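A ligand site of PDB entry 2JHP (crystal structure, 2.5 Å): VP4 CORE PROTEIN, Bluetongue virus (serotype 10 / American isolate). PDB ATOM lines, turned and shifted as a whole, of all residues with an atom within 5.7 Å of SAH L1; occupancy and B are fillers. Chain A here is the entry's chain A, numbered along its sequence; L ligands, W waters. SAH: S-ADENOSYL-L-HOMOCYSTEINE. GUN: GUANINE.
His 133 touches SAH L1 (O to N, 3.8 Å).
Glu 138 touches SAH L1 (OE2 to CA, 3.1 Å).
O of Lys 395 touches C2 of SAH L1 (3.6 Å).
CD1 of Leu 398 touches N6 of SAH L1 (3.6 Å).
Phe 410 touches SAH L1 (O to CG, 3.0 Å).
Tyr 411 touches SAH L1 (CD1 to C5, 3.4 Å).
Asn 414 touches SAH L1 (OD1 to C8, 3.3 Å).
Within 4 Å of SAH L1: Arg 122, His 133, Gly 134, Glu 136, Glu 138, Met 153, Lys 395, Asn 396, Gly 397, Leu 398, Leu 409, Phe 410, Tyr 411, Asn 414, Cys 416 and Asn 417.
The side-chain carboxylate (OE2) of Glu 138 is in hydrogen-bond range of the backbone NH (N) of Glu 136 (3.0 Å).
OD1 of Asn 417 sits close to SG of Cys 416 (3.3 Å).
O of Tyr 411 is in hydrogen-bond range of ND2 of Asn 417, at 3.1 Å.
The side-chain amide nitrogen (ND2) of Asn 417 sits at hydrogen-bond distance from the backbone carbonyl oxygen (O) of Leu 412 (2.8 Å).
The backbone NH (N) of Leu 398 is in hydrogen-bond range of the side-chain amide oxygen (OD1) of Asn 396.
OE2 of Glu 138 sits at hydrogen-bond distance from OG1 of Thr 139.
The side-chain amide nitrogen (ND2) of Asn 414 sits close to the backbone carbonyl oxygen (O) of Tyr 411 (3.4 Å).
O of Gly 152 sits at hydrogen-bond distance from N of Lys 395, 3.0 Å away.
O of Leu 409 lies within hydrogen-bond range of N of SAH L1, 2.5 Å away.
The side-chain carboxylate of Glu 136 is in hydrogen-bond range of an oxygen (O3') of SAH L1.
The side-chain amide oxygen of Asn 417 lies within hydrogen-bond range of a nitrogen (N6) of SAH L1 (2.8 Å).
NE of Arg 122 is in salt-bridge range of O of SAH L1 (2.9 Å).
O of Gly 134 sits at hydrogen-bond distance from N of SAH L1, 2.9 Å away.
The side-chain amide oxygen of Asn 396 lies close to a nitrogen (N1) of SAH L1, 3.0 Å away.
An oxygen (O2') of SAH L1 sits at hydrogen-bond distance from the backbone carbonyl oxygen (O) of Met 153 (3.0 Å).
N of Gly 397 is in hydrogen-bond range of N1 of SAH L1, at 3.2 Å.
SG of Cys 416 lies within hydrogen-bond range of N7 of SAH L1 (3.2 Å).
The guanidinium group (NH2) of Arg 122 lies close to a nitrogen (N9) of GUN L2 (3.4 Å).
Water W1 lies within hydrogen-bond range of the backbone NH (N) of Met 153, an oxygen (O3') of SAH L1 and the backbone carbonyl oxygen (O) of Ser 135.
Water W2 lies within hydrogen-bond range of OE1 of Glu 138 (2.5 Å), OXT of SAH L1 (2.9 Å) and N7 of GUN L2 (2.9 Å).
Water W3 lies within hydrogen-bond range of OG1 of Thr 139 (2.7 Å), OG of Ser 135 (3.1 Å) and N of SAH L1 (3.4 Å).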
ATOM      1  N   GLY A 118     -12.417 -41.839  21.152  1.00  0.00           N
ATOM      2  CA  GLY A 118     -12.826 -40.450  20.963  1.00  0.00           C
ATOM      3  C   GLY A 118     -14.334 -40.234  20.884  1.00  0.00           C
ATOM      4  O   GLY A 118     -14.822 -39.223  21.371  1.00  0.00           O
ATOM      5  N   ARG A 122     -16.908 -38.026  23.092  1.00  0.00           N
ATOM      6  CA  ARG A 122     -17.608 -36.953  22.421  1.00  0.00           C
ATOM      7  C   ARG A 122     -19.099 -37.053  22.629  1.00  0.00           C
ATOM      8  O   ARG A 122     -19.793 -36.032  22.709  1.00  0.00           O
ATOM      9  CB  ARG A 122     -17.275 -36.923  20.936  1.00  0.00           C
ATOM     10  CG  ARG A 122     -17.427 -35.531  20.318  1.00  0.00           C
ATOM     11  CD  ARG A 122     -17.058 -35.464  18.834  1.00  0.00           C
ATOM     12  NE  ARG A 122     -15.672 -35.871  18.622  1.00  0.00           N
ATOM     13  CZ  ARG A 122     -15.312 -37.086  18.248  1.00  0.00           C
ATOM     14  NH1 ARG A 122     -16.250 -37.997  18.024  1.00  0.00           N
ATOM     15  NH2 ARG A 122     -14.033 -37.379  18.095  1.00  0.00           N
ATOM     16  N   HIS A 133     -14.778 -26.854  21.141  1.00  0.00           N
ATOM     17  CA  HIS A 133     -13.578 -26.212  20.619  1.00  0.00           C
ATOM     18  C   HIS A 133     -12.604 -27.209  19.971  1.00  0.00           C
ATOM     19  O   HIS A 133     -12.669 -28.410  20.212  1.00  0.00           O
ATOM     20  CB  HIS A 133     -12.920 -25.358  21.706  1.00  0.00           C
ATOM     21  CG  HIS A 133     -13.805 -24.244  22.181  1.00  0.00           C
ATOM     22  ND1 HIS A 133     -13.748 -22.977  21.648  1.00  0.00           N
ATOM     23  CD2 HIS A 133     -14.786 -24.219  23.117  1.00  0.00           C
ATOM     24  CE1 HIS A 133     -14.649 -22.210  22.245  1.00  0.00           C
ATOM     25  NE2 HIS A 133     -15.291 -22.945  23.132  1.00  0.00           N
ATOM     26  N   GLY A 134     -11.725 -26.675  19.124  1.00  0.00           N
ATOM     27  CA  GLY A 134     -10.805 -27.445  18.281  1.00  0.00           C
ATOM     28  C   GLY A 134     -11.540 -28.400  17.353  1.00  0.00           C
ATOM     29  O   GLY A 134     -11.074 -29.519  17.107  1.00  0.00           O
ATOM     30  N   SER A 135     -12.677 -27.968  16.822  1.00  0.00           N
ATOM     31  CA  SER A 135     -13.581 -28.904  16.151  1.00  0.00           C
ATOM     32  C   SER A 135     -13.186 -29.076  14.722  1.00  0.00           C
ATOM     33  O   SER A 135     -12.500 -28.240  14.169  1.00  0.00           O
ATOM     34  CB  SER A 135     -15.042 -28.431  16.226  1.00  0.00           C
ATOM     35  OG  SER A 135     -15.478 -28.257  17.564  1.00  0.00           O
ATOM     36  N   GLU A 136     -13.638 -30.184  14.140  1.00  0.00           N
ATOM     37  CA  GLU A 136     -13.496 -30.447  12.708  1.00  0.00           C
ATOM     38  C   GLU A 136     -14.702 -31.248  12.281  1.00  0.00           C
ATOM     39  O   GLU A 136     -15.633 -31.404  13.072  1.00  0.00           O
ATOM     40  CB  GLU A 136     -12.213 -31.190  12.423  1.00  0.00           C
ATOM     41  CG  GLU A 136     -10.998 -30.338  12.324  1.00  0.00           C
ATOM     42  CD  GLU A 136      -9.828 -31.149  11.895  1.00  0.00           C
ATOM     43  OE1 GLU A 136     -10.017 -32.321  11.516  1.00  0.00           O
ATOM     44  OE2 GLU A 136      -8.706 -30.636  11.908  1.00  0.00           O
ATOM     45  N   GLU A 138     -15.697 -34.215  12.188  1.00  0.00           N
ATOM     46  CA  GLU A 138     -16.230 -35.231  13.128  1.00  0.00           C
ATOM     47  C   GLU A 138     -17.236 -34.661  14.143  1.00  0.00           C
ATOM     48  O   GLU A 138     -18.182 -35.348  14.534  1.00  0.00           O
ATOM     49  CB  GLU A 138     -15.117 -35.974  13.865  1.00  0.00           C
ATOM     50  CG  GLU A 138     -14.624 -35.286  15.129  1.00  0.00           C
ATOM     51  CD  GLU A 138     -13.810 -34.047  14.828  1.00  0.00           C
ATOM     52  OE1 GLU A 138     -12.785 -34.174  14.130  1.00  0.00           O
ATOM     53  OE2 GLU A 138     -14.177 -32.951  15.292  1.00  0.00           O
ATOM     54  N   THR A 139     -17.022 -33.405  14.553  1.00  0.00           N
ATOM     55  CA  THR A 139     -17.911 -32.771  15.509  1.00  0.00           C
ATOM     56  C   THR A 139     -19.183 -32.275  14.834  1.00  0.00           C
ATOM     57  O   THR A 139     -20.286 -32.523  15.323  1.00  0.00           O
ATOM     58  CB  THR A 139     -17.221 -31.646  16.296  1.00  0.00           C
ATOM     59  OG1 THR A 139     -16.032 -32.165  16.887  1.00  0.00           O
ATOM     60  CG2 THR A 139     -18.130 -31.149  17.408  1.00  0.00           C
ATOM     61  N   GLY A 152     -13.466 -23.948  16.268  1.00  0.00           N
ATOM     62  CA  GLY A 152     -12.196 -24.558  15.902  1.00  0.00           C
ATOM     63  C   GLY A 152     -11.335 -23.621  15.074  1.00  0.00           C
ATOM     64  O   GLY A 152     -11.670 -22.450  14.883  1.00  0.00           O
ATOM     65  N   MET A 153     -10.211 -24.153  14.612  1.00  0.00           N
ATOM     66  CA  MET A 153      -9.349 -23.448  13.653  1.00  0.00           C
ATOM     67  C   MET A 153      -8.906 -24.466  12.594  1.00  0.00           C
ATOM     68  O   MET A 153      -7.756 -24.900  12.570  1.00  0.00           O
ATOM     69  CB  MET A 153      -8.163 -22.806  14.364  1.00  0.00           C
ATOM     70  CG  MET A 153      -8.558 -21.949  15.542  1.00  0.00           C
ATOM     71  SD  MET A 153      -7.261 -20.859  16.084  1.00  0.00           S
ATOM     72  CE  MET A 153      -7.609 -19.412  15.069  1.00  0.00           C
ATOM     73  N   PRO A 154      -9.858 -24.891  11.744  1.00  0.00           N
ATOM     74  CA  PRO A 154      -9.559 -25.926  10.754  1.00  0.00           C
ATOM     75  C   PRO A 154      -8.727 -25.376   9.617  1.00  0.00           C
ATOM     76  O   PRO A 154      -8.717 -24.158   9.395  1.00  0.00           O
ATOM     77  CB  PRO A 154     -10.947 -26.350  10.265  1.00  0.00           C
ATOM     78  CG  PRO A 154     -11.802 -25.162  10.485  1.00  0.00           C
ATOM     79  CD  PRO A 154     -11.257 -24.446  11.669  1.00  0.00           C
ATOM     80  N   GLU A 155      -8.026 -26.272   8.912  1.00  0.00           N
ATOM     81  CA  GLU A 155      -7.096 -25.923   7.839  1.00  0.00           C
ATOM     82  C   GLU A 155      -7.894 -25.302   6.710  1.00  0.00           C
ATOM     83  O   GLU A 155      -8.768 -25.932   6.132  1.00  0.00           O
ATOM     84  CB  GLU A 155      -6.351 -27.182   7.341  1.00  0.00           C
ATOM     85  CG  GLU A 155      -4.835 -26.971   7.126  1.00  0.00           C
ATOM     86  CD  GLU A 155      -4.174 -28.033   6.214  1.00  0.00           C
ATOM     87  OE1 GLU A 155      -4.579 -29.224   6.236  1.00  0.00           O
ATOM     88  OE2 GLU A 155      -3.219 -27.672   5.467  1.00  0.00           O
ATOM     89  N   LYS A 395     -12.287 -19.709  16.029  1.00  0.00           N
ATOM     90  CA  LYS A 395     -12.023 -19.165  17.374  1.00  0.00           C
ATOM     91  C   LYS A 395     -10.958 -19.998  18.062  1.00  0.00           C
ATOM     92  O   LYS A 395     -10.986 -21.230  17.990  1.00  0.00           O
ATOM     93  CB  LYS A 395     -13.294 -19.247  18.241  1.00  0.00           C
ATOM     94  CG  LYS A 395     -13.605 -18.020  19.083  1.00  0.00           C
ATOM     95  CD  LYS A 395     -14.531 -17.090  18.318  1.00  0.00           C
ATOM     96  CE  LYS A 395     -15.147 -16.025  19.217  1.00  0.00           C
ATOM     97  NZ  LYS A 395     -16.307 -15.383  18.546  1.00  0.00           N
ATOM     98  N   ASN A 396     -10.009 -19.349  18.727  1.00  0.00           N
ATOM     99  CA  ASN A 396      -8.980 -20.042  19.496  1.00  0.00           C
ATOM    100  C   ASN A 396      -9.493 -20.404  20.888  1.00  0.00           C
ATOM    101  O   ASN A 396      -9.716 -19.530  21.739  1.00  0.00           O
ATOM    102  CB  ASN A 396      -7.689 -19.222  19.587  1.00  0.00           C
ATOM    103  CG  ASN A 396      -6.511 -20.014  20.180  1.00  0.00           C
ATOM    104  OD1 ASN A 396      -6.691 -20.923  21.003  1.00  0.00           O
ATOM    105  ND2 ASN A 396      -5.288 -19.647  19.773  1.00  0.00           N
ATOM    106  N   GLY A 397      -9.624 -21.710  21.124  1.00  0.00           N
ATOM    107  CA  GLY A 397     -10.174 -22.251  22.354  1.00  0.00           C
ATOM    108  C   GLY A 397      -9.572 -21.664  23.608  1.00  0.00           C
ATOM    109  O   GLY A 397     -10.304 -21.366  24.556  1.00  0.00           O
ATOM    110  N   LEU A 398      -8.255 -21.477  23.599  1.00  0.00           N
ATOM    111  CA  LEU A 398      -7.522 -20.993  24.771  1.00  0.00           C
ATOM    112  C   LEU A 398      -7.863 -19.540  25.068  1.00  0.00           C
ATOM    113  O   LEU A 398      -7.773 -19.114  26.220  1.00  0.00           O
ATOM    114  CB  LEU A 398      -6.017 -21.123  24.584  1.00  0.00           C
ATOM    115  CG  LEU A 398      -5.442 -22.483  24.186  1.00  0.00           C
ATOM    116  CD1 LEU A 398      -4.063 -22.313  23.573  1.00  0.00           C
ATOM    117  CD2 LEU A 398      -5.399 -23.422  25.379  1.00  0.00           C
ATOM    118  N   LEU A 409     -12.064 -31.267  23.304  1.00  0.00           N
ATOM    119  CA  LEU A 409     -11.603 -32.606  23.007  1.00  0.00           C
ATOM    120  C   LEU A 409     -10.500 -32.617  21.931  1.00  0.00           C
ATOM    121  O   LEU A 409     -10.665 -32.046  20.858  1.00  0.00           O
ATOM    122  CB  LEU A 409     -12.791 -33.484  22.618  1.00  0.00           C
ATOM    123  CG  LEU A 409     -13.876 -33.718  23.679  1.00  0.00           C
ATOM    124  CD1 LEU A 409     -15.145 -34.269  23.083  1.00  0.00           C
ATOM    125  CD2 LEU A 409     -13.363 -34.642  24.763  1.00  0.00           C
ATOM    126  N   PHE A 410      -9.375 -33.256  22.274  1.00  0.00           N
ATOM    127  CA  PHE A 410      -8.318 -33.617  21.342  1.00  0.00           C
ATOM    128  C   PHE A 410      -7.752 -32.439  20.549  1.00  0.00           C
ATOM    129  O   PHE A 410      -7.776 -32.452  19.320  1.00  0.00           O
ATOM    130  CB  PHE A 410      -8.770 -34.736  20.372  1.00  0.00           C
ATOM    131  CG  PHE A 410      -9.372 -35.929  21.037  1.00  0.00           C
ATOM    132  CD1 PHE A 410     -10.737 -36.140  20.960  1.00  0.00           C
ATOM    133  CD2 PHE A 410      -8.583 -36.833  21.718  1.00  0.00           C
ATOM    134  CE1 PHE A 410     -11.309 -37.241  21.571  1.00  0.00           C
ATOM    135  CE2 PHE A 410      -9.137 -37.948  22.321  1.00  0.00           C
ATOM    136  CZ  PHE A 410     -10.507 -38.146  22.262  1.00  0.00           C
ATOM    137  N   TYR A 411      -7.240 -31.434  21.256  1.00  0.00           N
ATOM    138  CA  TYR A 411      -6.637 -30.305  20.576  1.00  0.00           C
ATOM    139  C   TYR A 411      -5.628 -29.560  21.452  1.00  0.00           C
ATOM    140  O   TYR A 411      -4.599 -29.096  20.956  1.00  0.00           O
ATOM    141  CB  TYR A 411      -7.721 -29.346  20.023  1.00  0.00           C
ATOM    142  CG  TYR A 411      -8.262 -28.294  20.975  1.00  0.00           C
ATOM    143  CD1 TYR A 411      -7.608 -27.075  21.125  1.00  0.00           C
ATOM    144  CD2 TYR A 411      -9.437 -28.515  21.696  1.00  0.00           C
ATOM    145  CE1 TYR A 411      -8.111 -26.090  21.988  1.00  0.00           C
ATOM    146  CE2 TYR A 411      -9.957 -27.538  22.572  1.00  0.00           C
ATOM    147  CZ  TYR A 411      -9.290 -26.326  22.703  1.00  0.00           C
ATOM    148  OH  TYR A 411      -9.755 -25.364  23.570  1.00  0.00           O
ATOM    149  N   LEU A 412      -5.928 -29.465  22.743  1.00  0.00           N
ATOM    150  CA  LEU A 412      -5.074 -28.723  23.676  1.00  0.00           C
ATOM    151  C   LEU A 412      -3.560 -28.881  23.444  1.00  0.00           C
ATOM    152  O   LEU A 412      -2.855 -27.889  23.286  1.00  0.00           O
ATOM    153  CB  LEU A 412      -5.426 -29.104  25.110  1.00  0.00           C
ATOM    154  CG  LEU A 412      -6.396 -28.235  25.942  1.00  0.00           C
ATOM    155  CD1 LEU A 412      -6.950 -27.035  25.195  1.00  0.00           C
ATOM    156  CD2 LEU A 412      -7.514 -29.054  26.523  1.00  0.00           C
ATOM    157  N   ASN A 414      -1.940 -30.199  20.984  1.00  0.00           N
ATOM    158  CA  ASN A 414      -1.452 -30.042  19.619  1.00  0.00           C
ATOM    159  C   ASN A 414      -0.208 -29.145  19.642  1.00  0.00           C
ATOM    160  O   ASN A 414      -0.139 -28.203  20.438  1.00  0.00           O
ATOM    161  CB  ASN A 414      -2.510 -29.391  18.737  1.00  0.00           C
ATOM    162  CG  ASN A 414      -3.546 -30.383  18.206  1.00  0.00           C
ATOM    163  OD1 ASN A 414      -4.230 -30.081  17.220  1.00  0.00           O
ATOM    164  ND2 ASN A 414      -3.684 -31.545  18.850  1.00  0.00           N
ATOM    165  N   CYS A 416       0.874 -26.769  17.908  1.00  0.00           N
ATOM    166  CA  CYS A 416       0.620 -25.329  17.765  1.00  0.00           C
ATOM    167  C   CYS A 416       0.330 -24.604  19.084  1.00  0.00           C
ATOM    168  O   CYS A 416       0.243 -23.372  19.108  1.00  0.00           O
ATOM    169  CB  CYS A 416      -0.538 -25.102  16.790  1.00  0.00           C
ATOM    170  SG  CYS A 416      -2.149 -25.625  17.419  1.00  0.00           S
ATOM    171  N   ASN A 417       0.180 -25.352  20.176  1.00  0.00           N
ATOM    172  CA  ASN A 417      -0.100 -24.775  21.508  1.00  0.00           C
ATOM    173  C   ASN A 417       1.049 -24.941  22.511  1.00  0.00           C
ATOM    174  O   ASN A 417       0.882 -24.683  23.709  1.00  0.00           O
ATOM    175  CB  ASN A 417      -1.392 -25.366  22.093  1.00  0.00           C
ATOM    176  CG  ASN A 417      -2.568 -25.214  21.166  1.00  0.00           C
ATOM    177  OD1 ASN A 417      -2.640 -24.260  20.412  1.00  0.00           O
ATOM    178  ND2 ASN A 417      -3.493 -26.168  21.209  1.00  0.00           N
HETATM  179  N   SAH L   1     -11.919 -31.826  18.674  1.00  0.00           N
HETATM  180  CA  SAH L   1     -12.109 -32.827  17.577  1.00  0.00           C
HETATM  181  CB  SAH L   1     -10.978 -32.871  16.549  1.00  0.00           C
HETATM  182  CG  SAH L   1      -9.568 -32.454  16.937  1.00  0.00           C
HETATM  183  SD  SAH L   1      -8.537 -32.284  15.461  1.00  0.00           S
HETATM  184  C   SAH L   1     -12.440 -34.214  18.094  1.00  0.00           C
HETATM  185  O   SAH L   1     -13.229 -34.367  19.035  1.00  0.00           O
HETATM  186  OXT SAH L   1     -11.958 -35.224  17.576  1.00  0.00           O
HETATM  187  C5' SAH L   1      -7.687 -30.868  16.217  1.00  0.00           C
HETATM  188  C4' SAH L   1      -8.137 -29.539  15.643  1.00  0.00           C
HETATM  189  O4' SAH L   1      -8.070 -28.522  16.626  1.00  0.00           O
HETATM  190  C3' SAH L   1      -7.280 -29.076  14.474  1.00  0.00           C
HETATM  191  O3' SAH L   1      -8.169 -28.555  13.494  1.00  0.00           O
HETATM  192  C2' SAH L   1      -6.432 -27.944  15.039  1.00  0.00           C
HETATM  193  O2' SAH L   1      -6.163 -26.942  14.100  1.00  0.00           O
HETATM  194  C1' SAH L   1      -7.344 -27.404  16.140  1.00  0.00           C
HETATM  195  N9  SAH L   1      -6.607 -26.685  17.206  1.00  0.00           N
HETATM  196  C8  SAH L   1      -5.370 -26.997  17.716  1.00  0.00           C
HETATM  197  N7  SAH L   1      -5.057 -26.079  18.675  1.00  0.00           N
HETATM  198  C5  SAH L   1      -6.071 -25.190  18.773  1.00  0.00           C
HETATM  199  C6  SAH L   1      -6.280 -24.063  19.575  1.00  0.00           C
HETATM  200  N6  SAH L   1      -5.365 -23.701  20.472  1.00  0.00           N
HETATM  201  N1  SAH L   1      -7.447 -23.331  19.458  1.00  0.00           N
HETATM  202  C2  SAH L   1      -8.410 -23.718  18.538  1.00  0.00           C
HETATM  203  N3  SAH L   1      -8.211 -24.825  17.742  1.00  0.00           N
HETATM  204  C4  SAH L   1      -7.059 -25.556  17.849  1.00  0.00           C
HETATM  205  N9  GUN L   2     -11.493 -39.334  16.938  1.00  0.00           N
HETATM  206  C8  GUN L   2     -11.169 -38.328  16.130  1.00  0.00           C
HETATM  207  N7  GUN L   2      -9.910 -37.955  16.377  1.00  0.00           N
HETATM  208  C5  GUN L   2      -9.430 -38.718  17.353  1.00  0.00           C
HETATM  209  C6  GUN L   2      -8.199 -38.784  18.012  1.00  0.00           C
HETATM  210  O6  GUN L   2      -7.288 -38.014  17.714  1.00  0.00           O
HETATM  211  N1  GUN L   2      -8.007 -39.725  19.026  1.00  0.00           N
HETATM  212  C2  GUN L   2      -9.071 -40.591  19.340  1.00  0.00           C
HETATM  213  N2  GUN L   2      -8.926 -41.493  20.285  1.00  0.00           N
HETATM  214  N3  GUN L   2     -10.239 -40.506  18.696  1.00  0.00           N
HETATM  215  C4  GUN L   2     -10.441 -39.600  17.710  1.00  0.00           C
HETATM  216  O   HOH W   1      -9.973 -26.816  14.578  1.00  0.00           O
HETATM  217  O   HOH W   2     -10.927 -35.633  14.921  1.00  0.00           O
HETATM  218  O   HOH W   3     -15.173 -30.910  19.066  1.00  0.00           O
